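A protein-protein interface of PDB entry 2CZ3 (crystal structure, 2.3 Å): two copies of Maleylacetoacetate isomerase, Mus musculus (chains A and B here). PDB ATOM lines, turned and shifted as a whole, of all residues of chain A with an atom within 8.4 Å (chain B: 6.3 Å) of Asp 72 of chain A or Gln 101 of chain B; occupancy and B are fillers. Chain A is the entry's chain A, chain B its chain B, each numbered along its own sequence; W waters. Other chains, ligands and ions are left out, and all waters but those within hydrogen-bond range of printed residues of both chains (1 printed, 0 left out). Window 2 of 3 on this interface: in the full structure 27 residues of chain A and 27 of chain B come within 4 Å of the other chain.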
ATOM      1  N   GLY A  11     -28.556  28.237  10.472  1.00  0.00           N
ATOM      2  CA  GLY A  11     -29.139  27.782   9.173  1.00  0.00           C
ATOM      3  C   GLY A  11     -28.253  26.822   8.364  1.00  0.00           C
ATOM      4  O   GLY A  11     -28.746  25.817   7.827  1.00  0.00           O
ATOM      5  N   LYS A  12     -26.962  27.142   8.241  1.00  0.00           N
ATOM      6  CA  LYS A  12     -26.031  26.291   7.483  1.00  0.00           C
ATOM      7  C   LYS A  12     -24.787  25.894   8.304  1.00  0.00           C
ATOM      8  O   LYS A  12     -24.337  26.642   9.157  1.00  0.00           O
ATOM      9  CB  LYS A  12     -25.646  26.947   6.147  1.00  0.00           C
ATOM     10  CG  LYS A  12     -24.577  28.040   6.227  1.00  0.00           C
ATOM     11  CD  LYS A  12     -23.719  28.095   4.956  1.00  0.00           C
ATOM     12  CE  LYS A  12     -24.044  29.286   4.083  1.00  0.00           C
ATOM     13  NZ  LYS A  12     -23.030  29.437   2.985  1.00  0.00           N
ATOM     14  N   PRO A  13     -24.237  24.712   8.051  1.00  0.00           N
ATOM     15  CA  PRO A  13     -23.177  24.179   8.919  1.00  0.00           C
ATOM     16  C   PRO A  13     -21.994  25.127   9.099  1.00  0.00           C
ATOM     17  O   PRO A  13     -21.781  26.001   8.261  1.00  0.00           O
ATOM     18  CB  PRO A  13     -22.749  22.899   8.200  1.00  0.00           C
ATOM     19  CG  PRO A  13     -23.949  22.503   7.454  1.00  0.00           C
ATOM     20  CD  PRO A  13     -24.553  23.780   6.958  1.00  0.00           C
ATOM     21  N   ILE A  14     -21.265  24.966  10.202  1.00  0.00           N
ATOM     22  CA  ILE A  14     -20.128  25.815  10.533  1.00  0.00           C
ATOM     23  C   ILE A  14     -18.921  24.928  10.822  1.00  0.00           C
ATOM     24  O   ILE A  14     -18.911  24.151  11.769  1.00  0.00           O
ATOM     25  CB  ILE A  14     -20.419  26.695  11.766  1.00  0.00           C
ATOM     26  CG1 ILE A  14     -21.622  27.614  11.521  1.00  0.00           C
ATOM     27  CG2 ILE A  14     -19.206  27.528  12.109  1.00  0.00           C
ATOM     28  CD1 ILE A  14     -22.260  28.126  12.777  1.00  0.00           C
ATOM     29  N   ILE A  36     -21.835  19.372   0.454  1.00  0.00           N
ATOM     30  CA  ILE A  36     -22.420  20.164   1.537  1.00  0.00           C
ATOM     31  C   ILE A  36     -21.829  21.572   1.556  1.00  0.00           C
ATOM     32  O   ILE A  36     -20.632  21.752   1.674  1.00  0.00           O
ATOM     33  CB  ILE A  36     -22.188  19.517   2.917  1.00  0.00           C
ATOM     34  CG1 ILE A  36     -22.772  18.105   2.976  1.00  0.00           C
ATOM     35  CG2 ILE A  36     -22.810  20.391   4.022  1.00  0.00           C
ATOM     36  CD1 ILE A  36     -22.439  17.374   4.241  1.00  0.00           C
ATOM     37  N   LEU A  69     -17.320  20.953  13.988  1.00  0.00           N
ATOM     38  CA  LEU A  69     -18.350  21.106  12.973  1.00  0.00           C
ATOM     39  C   LEU A  69     -19.717  21.159  13.618  1.00  0.00           C
ATOM     40  O   LEU A  69     -20.114  20.236  14.321  1.00  0.00           O
ATOM     41  CB  LEU A  69     -18.284  19.985  11.925  1.00  0.00           C
ATOM     42  CG  LEU A  69     -19.361  20.054  10.828  1.00  0.00           C
ATOM     43  CD1 LEU A  69     -19.102  21.211   9.844  1.00  0.00           C
ATOM     44  CD2 LEU A  69     -19.492  18.721  10.092  1.00  0.00           C
ATOM     45  N   LYS A  70     -20.435  22.246  13.367  1.00  0.00           N
ATOM     46  CA  LYS A  70     -21.796  22.397  13.836  1.00  0.00           C
ATOM     47  C   LYS A  70     -22.724  21.991  12.696  1.00  0.00           C
ATOM     48  O   LYS A  70     -22.735  22.594  11.631  1.00  0.00           O
ATOM     49  CB  LYS A  70     -22.035  23.838  14.309  1.00  0.00           C
ATOM     50  CG  LYS A  70     -21.065  24.250  15.424  1.00  0.00           C
ATOM     51  CD  LYS A  70     -21.581  25.385  16.298  1.00  0.00           C
ATOM     52  CE  LYS A  70     -20.628  25.694  17.459  1.00  0.00           C
ATOM     53  NZ  LYS A  70     -20.459  27.145  17.691  1.00  0.00           N
ATOM     54  N   ILE A  71     -23.484  20.930  12.916  1.00  0.00           N
ATOM     55  CA  ILE A  71     -24.336  20.387  11.871  1.00  0.00           C
ATOM     56  C   ILE A  71     -25.496  19.595  12.465  1.00  0.00           C
ATOM     57  O   ILE A  71     -25.316  18.854  13.429  1.00  0.00           O
ATOM     58  CB  ILE A  71     -23.467  19.555  10.904  1.00  0.00           C
ATOM     59  CG1 ILE A  71     -24.248  19.196   9.649  1.00  0.00           C
ATOM     60  CG2 ILE A  71     -22.898  18.313  11.613  1.00  0.00           C
ATOM     61  CD1 ILE A  71     -23.397  18.656   8.579  1.00  0.00           C
ATOM     62  N   ASP A  72     -26.689  19.785  11.895  1.00  0.00           N
ATOM     63  CA  ASP A  72     -27.923  19.150  12.372  1.00  0.00           C
ATOM     64  C   ASP A  72     -28.179  19.403  13.852  1.00  0.00           C
ATOM     65  O   ASP A  72     -28.631  18.507  14.597  1.00  0.00           O
ATOM     66  CB  ASP A  72     -27.860  17.659  12.125  1.00  0.00           C
ATOM     67  CG  ASP A  72     -27.429  17.326  10.748  1.00  0.00           C
ATOM     68  OD1 ASP A  72     -27.665  18.133   9.814  1.00  0.00           O
ATOM     69  OD2 ASP A  72     -26.858  16.248  10.516  1.00  0.00           O
ATOM     70  N   GLY A  73     -27.870  20.623  14.275  1.00  0.00           N
ATOM     71  CA  GLY A  73     -28.057  21.046  15.652  1.00  0.00           C
ATOM     72  C   GLY A  73     -27.103  20.502  16.698  1.00  0.00           C
ATOM     73  O   GLY A  73     -27.346  20.667  17.884  1.00  0.00           O
ATOM     74  N   ILE A  74     -26.027  19.841  16.291  1.00  0.00           N
ATOM     75  CA  ILE A  74     -25.047  19.333  17.259  1.00  0.00           C
ATOM     76  C   ILE A  74     -23.635  19.722  16.884  1.00  0.00           C
ATOM     77  O   ILE A  74     -23.405  20.234  15.808  1.00  0.00           O
ATOM     78  CB  ILE A  74     -25.146  17.820  17.407  1.00  0.00           C
ATOM     79  CG1 ILE A  74     -24.748  17.110  16.100  1.00  0.00           C
ATOM     80  CG2 ILE A  74     -26.552  17.440  17.835  1.00  0.00           C
ATOM     81  CD1 ILE A  74     -24.385  15.604  16.285  1.00  0.00           C
ATOM     82  N   THR A  75     -22.703  19.479  17.802  1.00  0.00           N
ATOM     83  CA  THR A  75     -21.305  19.839  17.613  1.00  0.00           C
ATOM     84  C   THR A  75     -20.453  18.585  17.652  1.00  0.00           C
ATOM     85  O   THR A  75     -20.535  17.818  18.605  1.00  0.00           O
ATOM     86  CB  THR A  75     -20.809  20.836  18.703  1.00  0.00           C
ATOM     87  OG1 THR A  75     -21.466  22.095  18.563  1.00  0.00           O
ATOM     88  CG2 THR A  75     -19.341  21.201  18.497  1.00  0.00           C
ATOM     89  N   ILE A  76     -19.607  18.421  16.632  1.00  0.00           N
ATOM     90  CA  ILE A  76     -18.793  17.233  16.465  1.00  0.00           C
ATOM     91  C   ILE A  76     -17.323  17.622  16.351  1.00  0.00           C
ATOM     92  O   ILE A  76     -16.935  18.333  15.427  1.00  0.00           O
ATOM     93  CB  ILE A  76     -19.231  16.478  15.175  1.00  0.00           C
ATOM     94  CG1 ILE A  76     -20.745  16.290  15.141  1.00  0.00           C
ATOM     95  CG2 ILE A  76     -18.545  15.118  15.080  1.00  0.00           C
ATOM     96  CD1 ILE A  76     -21.234  15.601  13.879  1.00  0.00           C
ATOM     97  N   TYR A  85     -19.912  10.561  10.504  1.00  0.00           N
ATOM     98  CA  TYR A  85     -21.245  11.124  10.608  1.00  0.00           C
ATOM     99  C   TYR A  85     -21.707  11.555   9.231  1.00  0.00           C
ATOM    100  O   TYR A  85     -22.804  11.217   8.810  1.00  0.00           O
ATOM    101  CB  TYR A  85     -21.257  12.313  11.549  1.00  0.00           C
ATOM    102  CG  TYR A  85     -22.612  12.933  11.743  1.00  0.00           C
ATOM    103  CD1 TYR A  85     -23.503  12.435  12.704  1.00  0.00           C
ATOM    104  CD2 TYR A  85     -23.005  14.025  10.980  1.00  0.00           C
ATOM    105  CE1 TYR A  85     -24.759  13.019  12.891  1.00  0.00           C
ATOM    106  CE2 TYR A  85     -24.247  14.617  11.166  1.00  0.00           C
ATOM    107  CZ  TYR A  85     -25.109  14.111  12.127  1.00  0.00           C
ATOM    108  OH  TYR A  85     -26.318  14.700  12.290  1.00  0.00           O
ATOM    109  N   LEU A  86     -20.850  12.276   8.523  1.00  0.00           N
ATOM    110  CA  LEU A  86     -21.123  12.683   7.156  1.00  0.00           C
ATOM    111  C   LEU A  86     -21.425  11.483   6.263  1.00  0.00           C
ATOM    112  O   LEU A  86     -22.394  11.509   5.525  1.00  0.00           O
ATOM    113  CB  LEU A  86     -19.945  13.489   6.598  1.00  0.00           C
ATOM    114  CG  LEU A  86     -19.637  14.852   7.283  1.00  0.00           C
ATOM    115  CD1 LEU A  86     -18.541  15.585   6.517  1.00  0.00           C
ATOM    116  CD2 LEU A  86     -20.859  15.753   7.412  1.00  0.00           C
ATOM    117  N   GLU A  88     -22.676   8.619   7.043  1.00  0.00           N
ATOM    118  CA  GLU A  88     -23.959   8.014   7.436  1.00  0.00           C
ATOM    119  C   GLU A  88     -25.170   8.870   7.101  1.00  0.00           C
ATOM    120  O   GLU A  88     -26.237   8.355   6.812  1.00  0.00           O
ATOM    121  CB  GLU A  88     -23.967   7.713   8.938  1.00  0.00           C
ATOM    122  CG  GLU A  88     -23.130   6.492   9.290  1.00  0.00           C
ATOM    123  CD  GLU A  88     -22.774   6.397  10.758  1.00  0.00           C
ATOM    124  OE1 GLU A  88     -23.152   7.289  11.558  1.00  0.00           O
ATOM    125  OE2 GLU A  88     -22.099   5.418  11.110  1.00  0.00           O
ATOM    126  N   THR A  89     -25.006  10.180   7.127  1.00  0.00           N
ATOM    127  CA  THR A  89     -26.129  11.083   6.926  1.00  0.00           C
ATOM    128  C   THR A  89     -26.214  11.575   5.485  1.00  0.00           C
ATOM    129  O   THR A  89     -27.300  11.963   5.039  1.00  0.00           O
ATOM    130  CB  THR A  89     -26.014  12.262   7.857  1.00  0.00           C
ATOM    131  OG1 THR A  89     -24.723  12.843   7.698  1.00  0.00           O
ATOM    132  CG2 THR A  89     -26.080  11.833   9.316  1.00  0.00           C
ATOM    133  N   ARG A  90     -25.063  11.578   4.791  1.00  0.00           N
ATOM    134  CA  ARG A  90     -24.942  11.912   3.352  1.00  0.00           C
ATOM    135  C   ARG A  90     -24.143  10.791   2.657  1.00  0.00           C
ATOM    136  O   ARG A  90     -22.929  10.896   2.454  1.00  0.00           O
ATOM    137  CB  ARG A  90     -24.250  13.267   3.135  1.00  0.00           C
ATOM    138  CG  ARG A  90     -25.078  14.483   3.539  1.00  0.00           C
ATOM    139  CD  ARG A  90     -25.200  14.673   5.067  1.00  0.00           C
ATOM    140  NE  ARG A  90     -25.866  15.911   5.415  1.00  0.00           N
ATOM    141  CZ  ARG A  90     -26.043  16.338   6.652  1.00  0.00           C
ATOM    142  NH1 ARG A  90     -25.604  15.628   7.685  1.00  0.00           N
ATOM    143  NH2 ARG A  90     -26.658  17.499   6.856  1.00  0.00           N
ATOM    144  N   GLN B  98     -28.126   3.458  17.493  1.00  0.00           N
ATOM    145  CA  GLN B  98     -28.719   3.539  16.149  1.00  0.00           C
ATOM    146  C   GLN B  98     -28.831   4.966  15.639  1.00  0.00           C
ATOM    147  O   GLN B  98     -28.702   5.224  14.427  1.00  0.00           O
ATOM    148  CB  GLN B  98     -30.080   2.869  16.130  1.00  0.00           C
ATOM    149  CG  GLN B  98     -29.949   1.349  16.250  1.00  0.00           C
ATOM    150  CD  GLN B  98     -31.265   0.668  16.546  1.00  0.00           C
ATOM    151  OE1 GLN B  98     -32.041   0.400  15.635  1.00  0.00           O
ATOM    152  NE2 GLN B  98     -31.516   0.379  17.819  1.00  0.00           N
ATOM    153  N   ASP B  99     -29.087   5.892  16.558  1.00  0.00           N
ATOM    154  CA  ASP B  99     -29.232   7.297  16.209  1.00  0.00           C
ATOM    155  C   ASP B  99     -27.876   7.816  15.725  1.00  0.00           C
ATOM    156  O   ASP B  99     -26.900   7.765  16.467  1.00  0.00           O
ATOM    157  CB  ASP B  99     -29.711   8.104  17.419  1.00  0.00           C
ATOM    158  CG  ASP B  99     -29.936   9.604  17.105  1.00  0.00           C
ATOM    159  OD1 ASP B  99     -28.960  10.357  17.061  1.00  0.00           O
ATOM    160  OD2 ASP B  99     -31.051  10.143  16.940  1.00  0.00           O
ATOM    161  N   PRO B 100     -27.809   8.296  14.482  1.00  0.00           N
ATOM    162  CA  PRO B 100     -26.545   8.776  13.909  1.00  0.00           C
ATOM    163  C   PRO B 100     -25.846   9.808  14.785  1.00  0.00           C
ATOM    164  O   PRO B 100     -24.614   9.795  14.882  1.00  0.00           O
ATOM    165  CB  PRO B 100     -26.958   9.432  12.582  1.00  0.00           C
ATOM    166  CG  PRO B 100     -28.344   8.958  12.286  1.00  0.00           C
ATOM    167  CD  PRO B 100     -28.939   8.416  13.544  1.00  0.00           C
ATOM    168  N   GLN B 101     -26.629  10.685  15.407  1.00  0.00           N
ATOM    169  CA  GLN B 101     -26.076  11.760  16.230  1.00  0.00           C
ATOM    170  C   GLN B 101     -25.487  11.244  17.548  1.00  0.00           C
ATOM    171  O   GLN B 101     -24.448  11.716  17.994  1.00  0.00           O
ATOM    172  CB  GLN B 101     -27.096  12.883  16.459  1.00  0.00           C
ATOM    173  CG  GLN B 101     -27.321  13.704  15.207  1.00  0.00           C
ATOM    174  CD  GLN B 101     -28.190  14.909  15.411  1.00  0.00           C
ATOM    175  OE1 GLN B 101     -28.532  15.260  16.537  1.00  0.00           O
ATOM    176  NE2 GLN B 101     -28.523  15.573  14.326  1.00  0.00           N
ATOM    177  N   LYS B 102     -26.128  10.240  18.134  1.00  0.00           N
ATOM    178  CA  LYS B 102     -25.553   9.537  19.266  1.00  0.00           C
ATOM    179  C   LYS B 102     -24.270   8.772  18.873  1.00  0.00           C
ATOM    180  O   LYS B 102     -23.289   8.762  19.635  1.00  0.00           O
ATOM    181  CB  LYS B 102     -26.590   8.615  19.907  1.00  0.00           C
ATOM    182  CG  LYS B 102     -27.709   9.375  20.619  1.00  0.00           C
ATOM    183  CD  LYS B 102     -28.661   8.440  21.422  1.00  0.00           C
ATOM    184  CE  LYS B 102     -29.159   9.085  22.746  1.00  0.00           C
ATOM    185  NZ  LYS B 102     -30.633   9.407  22.733  1.00  0.00           N
ATOM    186  N   ARG B 103     -24.263   8.143  17.695  1.00  0.00           N
ATOM    187  CA  ARG B 103     -23.062   7.472  17.209  1.00  0.00           C
ATOM    188  C   ARG B 103     -21.904   8.468  17.041  1.00  0.00           C
ATOM    189  O   ARG B 103     -20.730   8.106  17.201  1.00  0.00           O
ATOM    190  CB  ARG B 103     -23.299   6.801  15.872  1.00  0.00           C
ATOM    191  CG  ARG B 103     -24.291   5.652  15.868  1.00  0.00           C
ATOM    192  CD  ARG B 103     -24.850   5.389  14.485  1.00  0.00           C
ATOM    193  NE  ARG B 103     -23.869   4.703  13.665  1.00  0.00           N
ATOM    194  CZ  ARG B 103     -23.753   3.386  13.594  1.00  0.00           C
ATOM    195  NH1 ARG B 103     -24.561   2.588  14.285  1.00  0.00           N
ATOM    196  NH2 ARG B 103     -22.832   2.851  12.806  1.00  0.00           N
ATOM    197  N   ALA B 104     -22.207   9.715  16.688  1.00  0.00           N
ATOM    198  CA  ALA B 104     -21.140  10.704  16.552  1.00  0.00           C
ATOM    199  C   ALA B 104     -20.517  11.017  17.910  1.00  0.00           C
ATOM    200  O   ALA B 104     -19.303  11.175  18.007  1.00  0.00           O
ATOM    201  CB  ALA B 104     -21.634  11.971  15.891  1.00  0.00           C
ATOM    202  N   ILE B 105     -21.338  11.108  18.951  1.00  0.00           N
ATOM    203  CA  ILE B 105     -20.840  11.399  20.282  1.00  0.00           C
ATOM    204  C   ILE B 105     -19.996  10.255  20.845  1.00  0.00           C
ATOM    205  O   ILE B 105     -18.974  10.478  21.479  1.00  0.00           O
ATOM    206  CB  ILE B 105     -22.003  11.712  21.238  1.00  0.00           C
ATOM    207  CG1 ILE B 105     -22.622  13.056  20.869  1.00  0.00           C
ATOM    208  CG2 ILE B 105     -21.525  11.732  22.697  1.00  0.00           C
ATOM    209  CD1 ILE B 105     -23.860  13.383  21.655  1.00  0.00           C
ATOM    210  N   VAL B 106     -20.407   9.028  20.587  1.00  0.00           N
ATOM    211  CA  VAL B 106     -19.630   7.871  20.984  1.00  0.00           C
ATOM    212  C   VAL B 106     -18.294   7.838  20.252  1.00  0.00           C
ATOM    213  O   VAL B 106     -17.269   7.555  20.849  1.00  0.00           O
ATOM    214  CB  VAL B 106     -20.397   6.592  20.685  1.00  0.00           C
ATOM    215  CG1 VAL B 106     -19.454   5.384  20.569  1.00  0.00           C
ATOM    216  CG2 VAL B 106     -21.447   6.377  21.771  1.00  0.00           C
HETATM  217  O   HOH W   1     -22.581   9.204  13.117  1.00  0.00           O
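CG2 of Ile 74 of chain A touches OE1 of Gln 101 of chain B, at 3.2 Å.
CD1 of Tyr 85 of chain A touches O of Pro 100 of chain B, 3.6 Å away.
Ala 104 of chain B touches Tyr 85 of chain A (CB to CD1, 3.7 Å).
The backbone carbonyl oxygen of Asp 72 of chain A is in hydrogen-bond range of the side-chain amide nitrogen of Gln 101 of chain B (2.9 Å).
The side-chain carboxylate (OE2) of Glu 88 of chain A is in salt-bridge range of the guanidinium group (NH2) of Arg 103 of chain B, 3.2 Å away.
The side-chain hydroxyl (OH) of Tyr 85 of chain A lies within hydrogen-bond range of the side-chain amide nitrogen (NE2) of Gln 101 of chain B.
NH1 of Arg 90 of chain A is in salt-bridge range of OD2 of Asp 72 of chain A (3.2 Å).
The backbone carbonyl oxygen of Tyr 85 of chain A sits at hydrogen-bond distance from the side-chain hydroxyl of Thr 89 of chain A, 2.8 Å away.
The side-chain carboxylate (OD2) of Asp 72 of chain A lies within hydrogen-bond range of the side-chain hydroxyl (OH) of Tyr 85 of chain A (2.4 Å).
The side-chain carboxylate (OD1) of Asp 99 of chain B is in hydrogen-bond range of the backbone NH (N) of Gln 101 of chain B (2.9 Å).
Water W1 lies within hydrogen-bond range of OE1 of Glu 88 of chain A (2.5 Å) and O of Pro 100 of chain B (2.8 Å).
Of chain B, only Gln 101 comes within 4 Å of Asp 72 of chain A.
Printed residues of chain B within 4 Å of Ile 74 of chain A: Gln 101 (3.2 Å).
Printed residues of chain B within 4 Å of Tyr 85 of chain A: Pro 100, Gln 101 and Ala 104.
Of the printed residues of chain B, Glu 88 of chain A touches Arg 103 (3.2 Å).
Arg 90 of chain A touches none of the printed residues of chain B.
Of chain A, only Tyr 85 comes within 4 Å of Pro 100 of chain B.
Gln 101 of chain B touches just these residues of chain A: Asp 72, Ile 74 and Tyr 85.
Of the printed residues of chain A, Arg 103 of chain B touches Glu 88 (3.2 Å).
Printed residues of chain A within 4 Å of Ala 104 of chain B: Tyr 85.
The nearest residue of chain A that does not touch Gln 101 of chain B is Ile 71 of chain A (4.7 Å).
The nearest printed residue of chain B that does not touch Tyr 85 of chain A is Lys 102 of chain B (6.1 Å).
No position is printed for both chains.
Hydrophobic or aromatic side chains of chain A that line the printed part of chain B: Ile 74 and Tyr 85.
Among the printed residues, Asp or Glu carboxylates within 4 Å of a Lys or Arg side-chain nitrogen of the other chain: Glu 88 of chain A with Arg 103 of chain B (3.2 Å).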
